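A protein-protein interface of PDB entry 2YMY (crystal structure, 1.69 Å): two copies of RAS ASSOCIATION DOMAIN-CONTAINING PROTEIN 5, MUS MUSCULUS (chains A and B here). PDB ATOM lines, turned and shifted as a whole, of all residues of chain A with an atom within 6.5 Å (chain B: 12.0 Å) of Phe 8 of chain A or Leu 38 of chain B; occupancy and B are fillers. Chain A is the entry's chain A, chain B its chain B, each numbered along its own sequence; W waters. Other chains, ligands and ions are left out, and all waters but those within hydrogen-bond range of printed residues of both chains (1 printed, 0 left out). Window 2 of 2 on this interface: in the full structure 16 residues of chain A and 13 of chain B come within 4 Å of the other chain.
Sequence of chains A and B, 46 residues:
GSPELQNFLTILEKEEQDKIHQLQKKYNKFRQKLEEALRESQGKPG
The side-chain hydroxyl (OG) of Ser 2 of chain A sits at hydrogen-bond distance from the backbone NH (N) of Leu 5 of chain A. The guanidinium group (NH2) of Arg 31 of chain B lies within hydrogen-bond range of the side-chain amide oxygen (OD1) of Asn 28 of chain B, at 3.1 Å.
CD1 of Leu 5 of chain A touches CD2 of Leu 38 of chain B, 3.6 Å away. CD2 of Leu 38 of chain B touches CD2 of Phe 8 of chain A, at 3.4 Å. Leu 34 of chain B touches Leu 9 of chain A. Glu 35 of chain B touches Leu 9 of chain A. Leu 12 of chain A touches Tyr 27 of chain B. Leu 12 of chain A touches Phe 30 of chain B. Leu 12 of chain A touches Arg 31 of chain B (CD1 to N, 3.7 Å). Leu 34 of chain B touches Leu 12 of chain A. NH1 of Arg 31 of chain B touches CG of Glu 13 of chain A, at 3.96 Å.
Of chain B, only Leu 38 comes within 4 Å of Phe 8 of chain A. Leu 38 of chain B touches just these residues of chain A: Leu 5 and Phe 8. No residue of chain B comes within 4 Å of Glu 4 of chain A. Of chain B, only Leu 38 (3.6 Å) comes within 4 Å of Leu 5 of chain A. No residue of chain B comes within 4 Å of Asn 7 of chain A. No residue of chain B comes within 4 Å of Thr 10 of chain A. Ile 11 of chain A touches none of the printed residues of chain B. Printed residues of chain A within 4 Å of Leu 34 of chain B: Leu 9 and Leu 12. Of the printed residues of chain A, Tyr 27 of chain B touches Leu 12. Ala 37 of chain B touches none of the printed residues of chain A. The nearest printed residue of chain B that does not touch Leu 9 of chain A is Arg 31 of chain B (4.1 Å).
Hydrophobic or aromatic side chains of chain A that line the printed part of chain B: Leu 5, Phe 8, Leu 9 and Leu 12. Of the 15 printed residues of chain B, 6 touch a printed residue of chain A. Hydrophobic or aromatic side chains of chain B that line the printed part of chain A: Tyr 27, Phe 30, Leu 34 and Leu 38. Among the printed residues, no Asp or Glu carboxylate lies within 4 Å of a Lys or Arg side-chain nitrogen of the other chain.
No position is printed for both chains.
Water W1 lies within hydrogen-bond range of NH1 of Arg 31 of chain B (2.4 Å) and O of Leu 12 of chain A (3.3 Å).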
ATOM      1  N   SER A   2      -8.935   6.757  11.567  1.00  0.00           N
ATOM      2  CA  SER A   2      -7.992   6.008  12.386  1.00  0.00           C
ATOM      3  C   SER A   2      -7.973   4.544  11.975  1.00  0.00           C
ATOM      4  O   SER A   2      -8.877   4.080  11.275  1.00  0.00           O
ATOM      5  CB  SER A   2      -8.382   6.094  13.860  1.00  0.00           C
ATOM      6  OG  SER A   2      -9.564   5.348  14.112  1.00  0.00           O
ATOM      7  N   PRO A   3      -6.936   3.813  12.416  1.00  0.00           N
ATOM      8  CA  PRO A   3      -6.806   2.358  12.269  1.00  0.00           C
ATOM      9  C   PRO A   3      -7.980   1.579  12.876  1.00  0.00           C
ATOM     10  O   PRO A   3      -8.527   0.683  12.222  1.00  0.00           O
ATOM     11  CB  PRO A   3      -5.512   2.053  13.033  1.00  0.00           C
ATOM     12  CG  PRO A   3      -4.704   3.297  12.897  1.00  0.00           C
ATOM     13  CD  PRO A   3      -5.695   4.427  12.921  1.00  0.00           C
ATOM     14  N   GLU A   4      -8.346   1.910  14.116  1.00  0.00           N
ATOM     15  CA  GLU A   4      -9.475   1.267  14.771  1.00  0.00           C
ATOM     16  C   GLU A   4     -10.697   1.418  13.881  1.00  0.00           C
ATOM     17  O   GLU A   4     -11.481   0.478  13.730  1.00  0.00           O
ATOM     18  CB  GLU A   4      -9.765   1.890  16.143  1.00  0.00           C
ATOM     19  CG  GLU A   4      -8.697   1.642  17.201  1.00  0.00           C
ATOM     20  CD  GLU A   4      -7.886   2.891  17.521  1.00  0.00           C
ATOM     21  OE1 GLU A   4      -7.888   3.836  16.696  1.00  0.00           O
ATOM     22  OE2 GLU A   4      -7.243   2.926  18.597  1.00  0.00           O
ATOM     23  N   LEU A   5     -10.863   2.600  13.288  1.00  0.00           N
ATOM     24  CA  LEU A   5     -12.027   2.827  12.430  1.00  0.00           C
ATOM     25  C   LEU A   5     -11.978   1.891  11.228  1.00  0.00           C
ATOM     26  O   LEU A   5     -12.992   1.256  10.878  1.00  0.00           O
ATOM     27  CB  LEU A   5     -12.122   4.285  11.958  1.00  0.00           C
ATOM     28  CG  LEU A   5     -13.447   4.608  11.246  1.00  0.00           C
ATOM     29  CD1 LEU A   5     -14.620   4.439  12.209  1.00  0.00           C
ATOM     30  CD2 LEU A   5     -13.461   6.005  10.649  1.00  0.00           C
ATOM     31  N   GLN A   6     -10.804   1.795  10.599  1.00  0.00           N
ATOM     32  CA  GLN A   6     -10.655   0.942   9.415  1.00  0.00           C
ATOM     33  C   GLN A   6     -10.949  -0.508   9.781  1.00  0.00           C
ATOM     34  O   GLN A   6     -11.704  -1.187   9.077  1.00  0.00           O
ATOM     35  CB  GLN A   6      -9.253   1.036   8.787  1.00  0.00           C
ATOM     36  CG  GLN A   6      -8.639   2.442   8.695  1.00  0.00           C
ATOM     37  CD  GLN A   6      -9.406   3.405   7.795  1.00  0.00           C
ATOM     38  OE1 GLN A   6     -10.634   3.343   7.682  1.00  0.00           O
ATOM     39  NE2 GLN A   6      -8.674   4.313   7.153  1.00  0.00           N
ATOM     40  N   ASN A   7     -10.367  -0.976  10.883  1.00  0.00           N
ATOM     41  CA  ASN A   7     -10.574  -2.343  11.327  1.00  0.00           C
ATOM     42  C   ASN A   7     -12.062  -2.562  11.528  1.00  0.00           C
ATOM     43  O   ASN A   7     -12.649  -3.497  10.970  1.00  0.00           O
ATOM     44  CB  ASN A   7      -9.820  -2.632  12.631  1.00  0.00           C
ATOM     45  CG  ASN A   7     -10.058  -4.047  13.139  1.00  0.00           C
ATOM     46  OD1 ASN A   7      -9.949  -5.018  12.385  1.00  0.00           O
ATOM     47  ND2 ASN A   7     -10.412  -4.168  14.413  1.00  0.00           N
ATOM     48  N   PHE A   8     -12.703  -1.655  12.264  1.00  0.00           N
ATOM     49  CA  PHE A   8     -14.078  -1.928  12.659  1.00  0.00           C
ATOM     50  C   PHE A   8     -15.012  -1.815  11.460  1.00  0.00           C
ATOM     51  O   PHE A   8     -15.966  -2.586  11.329  1.00  0.00           O
ATOM     52  CB  PHE A   8     -14.538  -0.972  13.762  1.00  0.00           C
ATOM     53  CG  PHE A   8     -13.955  -1.253  15.108  1.00  0.00           C
ATOM     54  CD1 PHE A   8     -13.212  -2.384  15.368  1.00  0.00           C
ATOM     55  CD2 PHE A   8     -14.140  -0.340  16.135  1.00  0.00           C
ATOM     56  CE1 PHE A   8     -12.671  -2.599  16.610  1.00  0.00           C
ATOM     57  CE2 PHE A   8     -13.609  -0.559  17.379  1.00  0.00           C
ATOM     58  CZ  PHE A   8     -12.872  -1.682  17.619  1.00  0.00           C
ATOM     59  N   LEU A   9     -14.780  -0.845  10.579  1.00  0.00           N
ATOM     60  CA  LEU A   9     -15.662  -0.721   9.426  1.00  0.00           C
ATOM     61  C   LEU A   9     -15.511  -1.939   8.521  1.00  0.00           C
ATOM     62  O   LEU A   9     -16.505  -2.405   7.952  1.00  0.00           O
ATOM     63  CB  LEU A   9     -15.410   0.568   8.641  1.00  0.00           C
ATOM     64  CG  LEU A   9     -15.872   1.857   9.306  1.00  0.00           C
ATOM     65  CD1 LEU A   9     -15.496   3.056   8.447  1.00  0.00           C
ATOM     66  CD2 LEU A   9     -17.341   1.832   9.548  1.00  0.00           C
ATOM     67  N   THR A  10     -14.299  -2.443   8.319  1.00  0.00           N
ATOM     68  CA  THR A  10     -14.164  -3.634   7.456  1.00  0.00           C
ATOM     69  C   THR A  10     -14.798  -4.879   8.061  1.00  0.00           C
ATOM     70  O   THR A  10     -15.272  -5.768   7.330  1.00  0.00           O
ATOM     71  CB  THR A  10     -12.703  -3.956   7.111  1.00  0.00           C
ATOM     72  OG1 THR A  10     -12.031  -4.393   8.292  1.00  0.00           O
ATOM     73  CG2 THR A  10     -11.995  -2.731   6.528  1.00  0.00           C
ATOM     74  N   ILE A  11     -14.805  -4.974   9.381  1.00  0.00           N
ATOM     75  CA  ILE A  11     -15.550  -6.023  10.065  1.00  0.00           C
ATOM     76  C   ILE A  11     -17.034  -5.947   9.692  1.00  0.00           C
ATOM     77  O   ILE A  11     -17.639  -6.955   9.342  1.00  0.00           O
ATOM     78  CB  ILE A  11     -15.334  -5.950  11.589  1.00  0.00           C
ATOM     79  CG1 ILE A  11     -13.894  -6.354  11.911  1.00  0.00           C
ATOM     80  CG2 ILE A  11     -16.247  -6.873  12.301  1.00  0.00           C
ATOM     81  CD1 ILE A  11     -13.485  -6.033  13.322  1.00  0.00           C
ATOM     82  N   LEU A  12     -17.605  -4.744   9.760  1.00  0.00           N
ATOM     83  CA  LEU A  12     -19.012  -4.543   9.466  1.00  0.00           C
ATOM     84  C   LEU A  12     -19.285  -4.856   8.006  1.00  0.00           C
ATOM     85  O   LEU A  12     -20.322  -5.437   7.671  1.00  0.00           O
ATOM     86  CB  LEU A  12     -19.404  -3.088   9.730  1.00  0.00           C
ATOM     87  CG  LEU A  12     -20.244  -2.673  10.937  1.00  0.00           C
ATOM     88  CD1 LEU A  12     -21.095  -1.434  10.562  1.00  0.00           C
ATOM     89  CD2 LEU A  12     -21.126  -3.795  11.419  1.00  0.00           C
ATOM     90  N   GLU A  13     -18.391  -4.432   7.118  1.00  0.00           N
ATOM     91  CA  GLU A  13     -18.595  -4.660   5.684  1.00  0.00           C
ATOM     92  C   GLU A  13     -18.611  -6.168   5.422  1.00  0.00           C
ATOM     93  O   GLU A  13     -19.460  -6.654   4.653  1.00  0.00           O
ATOM     94  CB  GLU A  13     -17.492  -3.974   4.863  1.00  0.00           C
ATOM     95  CG  GLU A  13     -17.633  -2.454   4.835  1.00  0.00           C
ATOM     96  CD  GLU A  13     -16.375  -1.711   4.413  1.00  0.00           C
ATOM     97  OE1 GLU A  13     -15.441  -2.342   3.861  1.00  0.00           O
ATOM     98  OE2 GLU A  13     -16.330  -0.474   4.646  1.00  0.00           O
ATOM     99  N   TYR B  27     -27.516  -2.122   8.243  1.00  0.00           N
ATOM    100  CA  TYR B  27     -26.080  -1.957   8.257  1.00  0.00           C
ATOM    101  C   TYR B  27     -25.677  -0.541   7.911  1.00  0.00           C
ATOM    102  O   TYR B  27     -24.684  -0.025   8.423  1.00  0.00           O
ATOM    103  CB  TYR B  27     -25.434  -2.972   7.312  1.00  0.00           C
ATOM    104  CG  TYR B  27     -25.152  -4.267   8.027  1.00  0.00           C
ATOM    105  CD1 TYR B  27     -24.074  -4.365   8.884  1.00  0.00           C
ATOM    106  CD2 TYR B  27     -25.980  -5.350   7.893  1.00  0.00           C
ATOM    107  CE1 TYR B  27     -23.809  -5.509   9.567  1.00  0.00           C
ATOM    108  CE2 TYR B  27     -25.708  -6.533   8.579  1.00  0.00           C
ATOM    109  CZ  TYR B  27     -24.628  -6.589   9.412  1.00  0.00           C
ATOM    110  OH  TYR B  27     -24.313  -7.731  10.112  1.00  0.00           O
ATOM    111  N   ASN B  28     -26.480   0.143   7.074  1.00  0.00           N
ATOM    112  CA  ASN B  28     -26.192   1.562   6.843  1.00  0.00           C
ATOM    113  C   ASN B  28     -26.345   2.399   8.110  1.00  0.00           C
ATOM    114  O   ASN B  28     -25.511   3.250   8.383  1.00  0.00           O
ATOM    115  CB  ASN B  28     -27.063   2.133   5.734  1.00  0.00           C
ATOM    116  CG  ASN B  28     -26.745   1.522   4.381  1.00  0.00           C
ATOM    117  OD1 ASN B  28     -25.671   0.953   4.171  1.00  0.00           O
ATOM    118  ND2 ASN B  28     -27.696   1.627   3.455  1.00  0.00           N
ATOM    119  N   LYS B  29     -27.400   2.146   8.877  1.00  0.00           N
ATOM    120  CA  LYS B  29     -27.549   2.831  10.149  1.00  0.00           C
ATOM    121  C   LYS B  29     -26.406   2.441  11.111  1.00  0.00           C
ATOM    122  O   LYS B  29     -25.840   3.282  11.841  1.00  0.00           O
ATOM    123  CB  LYS B  29     -28.879   2.472  10.767  1.00  0.00           C
ATOM    124  CG  LYS B  29     -29.094   3.120  12.112  1.00  0.00           C
ATOM    125  CD  LYS B  29     -28.886   4.636  12.013  1.00  0.00           C
ATOM    126  CE  LYS B  29     -29.815   5.293  11.000  1.00  0.00           C
ATOM    127  NZ  LYS B  29     -29.849   6.772  11.191  1.00  0.00           N
ATOM    128  N   PHE B  30     -26.061   1.152  11.126  1.00  0.00           N
ATOM    129  CA  PHE B  30     -25.034   0.643  12.035  1.00  0.00           C
ATOM    130  C   PHE B  30     -23.700   1.332  11.741  1.00  0.00           C
ATOM    131  O   PHE B  30     -23.001   1.766  12.635  1.00  0.00           O
ATOM    132  CB  PHE B  30     -24.968  -0.887  11.854  1.00  0.00           C
ATOM    133  CG  PHE B  30     -24.156  -1.630  12.895  1.00  0.00           C
ATOM    134  CD1 PHE B  30     -23.423  -0.989  13.858  1.00  0.00           C
ATOM    135  CD2 PHE B  30     -24.110  -3.012  12.860  1.00  0.00           C
ATOM    136  CE1 PHE B  30     -22.664  -1.722  14.785  1.00  0.00           C
ATOM    137  CE2 PHE B  30     -23.366  -3.721  13.786  1.00  0.00           C
ATOM    138  CZ  PHE B  30     -22.654  -3.050  14.756  1.00  0.00           C
ATOM    139  N   ARG B  31     -23.367   1.442  10.461  1.00  0.00           N
ATOM    140  CA  ARG B  31     -22.179   2.114   9.990  1.00  0.00           C
ATOM    141  C   ARG B  31     -22.126   3.562  10.487  1.00  0.00           C
ATOM    142  O   ARG B  31     -21.117   4.021  11.027  1.00  0.00           O
ATOM    143  CB  ARG B  31     -22.217   2.106   8.468  1.00  0.00           C
ATOM    144  CG  ARG B  31     -20.951   2.527   7.813  1.00  0.00           C
ATOM    145  CD  ARG B  31     -21.035   2.392   6.283  1.00  0.00           C
ATOM    146  NE  ARG B  31     -22.124   1.534   5.815  1.00  0.00           N
ATOM    147  CZ  ARG B  31     -22.029   0.222   5.602  1.00  0.00           C
ATOM    148  NH1 ARG B  31     -20.890  -0.423   5.828  1.00  0.00           N
ATOM    149  NH2 ARG B  31     -23.082  -0.452   5.161  1.00  0.00           N
ATOM    150  N   GLN B  32     -23.234   4.255  10.305  1.00  0.00           N
ATOM    151  CA  GLN B  32     -23.312   5.646  10.740  1.00  0.00           C
ATOM    152  C   GLN B  32     -23.022   5.760  12.224  1.00  0.00           C
ATOM    153  O   GLN B  32     -22.235   6.610  12.653  1.00  0.00           O
ATOM    154  CB  GLN B  32     -24.693   6.199  10.479  1.00  0.00           C
ATOM    155  CG  GLN B  32     -24.812   7.642  10.951  1.00  0.00           C
ATOM    156  CD  GLN B  32     -26.237   8.141  10.895  1.00  0.00           C
ATOM    157  OE1 GLN B  32     -27.182   7.381  11.110  1.00  0.00           O
ATOM    158  NE2 GLN B  32     -26.401   9.419  10.594  1.00  0.00           N
ATOM    159  N   LYS B  33     -23.698   4.962  13.033  1.00  0.00           N
ATOM    160  CA  LYS B  33     -23.559   5.073  14.480  1.00  0.00           C
ATOM    161  C   LYS B  33     -22.246   4.540  14.988  1.00  0.00           C
ATOM    162  O   LYS B  33     -21.748   5.002  16.037  1.00  0.00           O
ATOM    163  CB  LYS B  33     -24.704   4.372  15.189  1.00  0.00           C
ATOM    164  CG  LYS B  33     -26.068   4.928  14.804  1.00  0.00           C
ATOM    165  CD  LYS B  33     -26.224   6.424  15.134  1.00  0.00           C
ATOM    166  CE  LYS B  33     -27.520   7.028  14.650  1.00  0.00           C
ATOM    167  NZ  LYS B  33     -27.537   8.558  14.889  1.00  0.00           N
ATOM    168  N   LEU B  34     -21.671   3.561  14.266  1.00  0.00           N
ATOM    169  CA  LEU B  34     -20.361   3.051  14.642  1.00  0.00           C
ATOM    170  C   LEU B  34     -19.293   4.141  14.481  1.00  0.00           C
ATOM    171  O   LEU B  34     -18.433   4.356  15.355  1.00  0.00           O
ATOM    172  CB  LEU B  34     -20.023   1.842  13.752  1.00  0.00           C
ATOM    173  CG  LEU B  34     -18.625   1.320  13.769  1.00  0.00           C
ATOM    174  CD1 LEU B  34     -18.293   0.904  15.142  1.00  0.00           C
ATOM    175  CD2 LEU B  34     -18.585   0.131  12.786  1.00  0.00           C
ATOM    176  N   GLU B  35     -19.384   4.861  13.376  1.00  0.00           N
ATOM    177  CA  GLU B  35     -18.469   5.965  13.127  1.00  0.00           C
ATOM    178  C   GLU B  35     -18.586   7.043  14.217  1.00  0.00           C
ATOM    179  O   GLU B  35     -17.569   7.553  14.729  1.00  0.00           O
ATOM    180  CB  GLU B  35     -18.723   6.521  11.729  1.00  0.00           C
ATOM    181  CG  GLU B  35     -18.350   5.511  10.624  1.00  0.00           C
ATOM    182  CD  GLU B  35     -18.456   6.071   9.210  1.00  0.00           C
ATOM    183  OE1 GLU B  35     -19.580   6.102   8.659  1.00  0.00           O
ATOM    184  OE2 GLU B  35     -17.408   6.462   8.644  1.00  0.00           O
ATOM    185  N   GLU B  36     -19.815   7.345  14.614  1.00  0.00           N
ATOM    186  CA  GLU B  36     -20.057   8.315  15.678  1.00  0.00           C
ATOM    187  C   GLU B  36     -19.449   7.800  16.961  1.00  0.00           C
ATOM    188  O   GLU B  36     -18.776   8.543  17.670  1.00  0.00           O
ATOM    189  CB  GLU B  36     -21.558   8.580  15.902  1.00  0.00           C
ATOM    190  CG  GLU B  36     -21.898   9.401  17.168  1.00  0.00           C
ATOM    191  CD  GLU B  36     -23.387   9.795  17.296  1.00  0.00           C
ATOM    192  OE1 GLU B  36     -24.188   9.412  16.424  1.00  0.00           O
ATOM    193  OE2 GLU B  36     -23.767  10.496  18.277  1.00  0.00           O
ATOM    194  N   ALA B  37     -19.696   6.526  17.284  1.00  0.00           N
ATOM    195  CA  ALA B  37     -19.269   6.016  18.589  1.00  0.00           C
ATOM    196  C   ALA B  37     -17.765   6.048  18.701  1.00  0.00           C
ATOM    197  O   ALA B  37     -17.221   6.275  19.790  1.00  0.00           O
ATOM    198  CB  ALA B  37     -19.782   4.590  18.829  1.00  0.00           C
ATOM    199  N   LEU B  38     -17.098   5.824  17.581  1.00  0.00           N
ATOM    200  CA  LEU B  38     -15.641   5.751  17.609  1.00  0.00           C
ATOM    201  C   LEU B  38     -15.094   7.147  17.850  1.00  0.00           C
ATOM    202  O   LEU B  38     -14.226   7.336  18.708  1.00  0.00           O
ATOM    203  CB  LEU B  38     -15.099   5.236  16.299  1.00  0.00           C
ATOM    204  CG  LEU B  38     -13.909   4.260  16.328  1.00  0.00           C
ATOM    205  CD1 LEU B  38     -13.464   3.849  17.727  1.00  0.00           C
ATOM    206  CD2 LEU B  38     -14.290   3.027  15.546  1.00  0.00           C
ATOM    207  N   ARG B  39     -15.585   8.127  17.078  1.00  0.00           N
ATOM    208  CA  ARG B  39     -15.148   9.535  17.221  1.00  0.00           C
ATOM    209  C   ARG B  39     -15.246   9.958  18.668  1.00  0.00           C
ATOM    210  O   ARG B  39     -14.283  10.444  19.258  1.00  0.00           O
ATOM    211  CB  ARG B  39     -15.981  10.497  16.357  1.00  0.00           C
ATOM    212  CG  ARG B  39     -15.766  12.034  16.648  1.00  0.00           C
ATOM    213  CD  ARG B  39     -17.123  12.801  16.693  1.00  0.00           C
ATOM    214  NE  ARG B  39     -17.092  14.278  16.629  1.00  0.00           N
ATOM    215  CZ  ARG B  39     -17.104  15.103  17.685  1.00  0.00           C
ATOM    216  NH1 ARG B  39     -17.090  14.607  18.914  1.00  0.00           N
ATOM    217  NH2 ARG B  39     -17.123  16.430  17.513  1.00  0.00           N
ATOM    218  N   GLU B  40     -16.415   9.736  19.247  1.00  0.00           N
ATOM    219  CA  GLU B  40     -16.701  10.200  20.589  1.00  0.00           C
ATOM    220  C   GLU B  40     -16.065   9.340  21.668  1.00  0.00           C
ATOM    221  O   GLU B  40     -16.234   9.626  22.848  1.00  0.00           O
ATOM    222  CB  GLU B  40     -18.216  10.290  20.776  1.00  0.00           C
ATOM    223  CG  GLU B  40     -18.811  11.109  19.662  1.00  0.00           C
ATOM    224  CD  GLU B  40     -20.321  11.324  19.759  1.00  0.00           C
ATOM    225  OE1 GLU B  40     -21.005  10.684  20.596  1.00  0.00           O
ATOM    226  OE2 GLU B  40     -20.789  12.187  18.993  1.00  0.00           O
ATOM    227  N   SER B  41     -15.337   8.300  21.261  1.00  0.00           N
ATOM    228  CA  SER B  41     -14.516   7.520  22.191  1.00  0.00           C
ATOM    229  C   SER B  41     -13.043   7.958  22.202  1.00  0.00           C
ATOM    230  O   SER B  41     -12.386   8.051  21.157  1.00  0.00           O
ATOM    231  CB  SER B  41     -14.625   6.029  21.855  1.00  0.00           C
ATOM    232  OG  SER B  41     -15.835   5.499  22.371  1.00  0.00           O
HETATM  233  O   HOH W   1     -21.667  -2.658   6.372  1.00  0.00           O
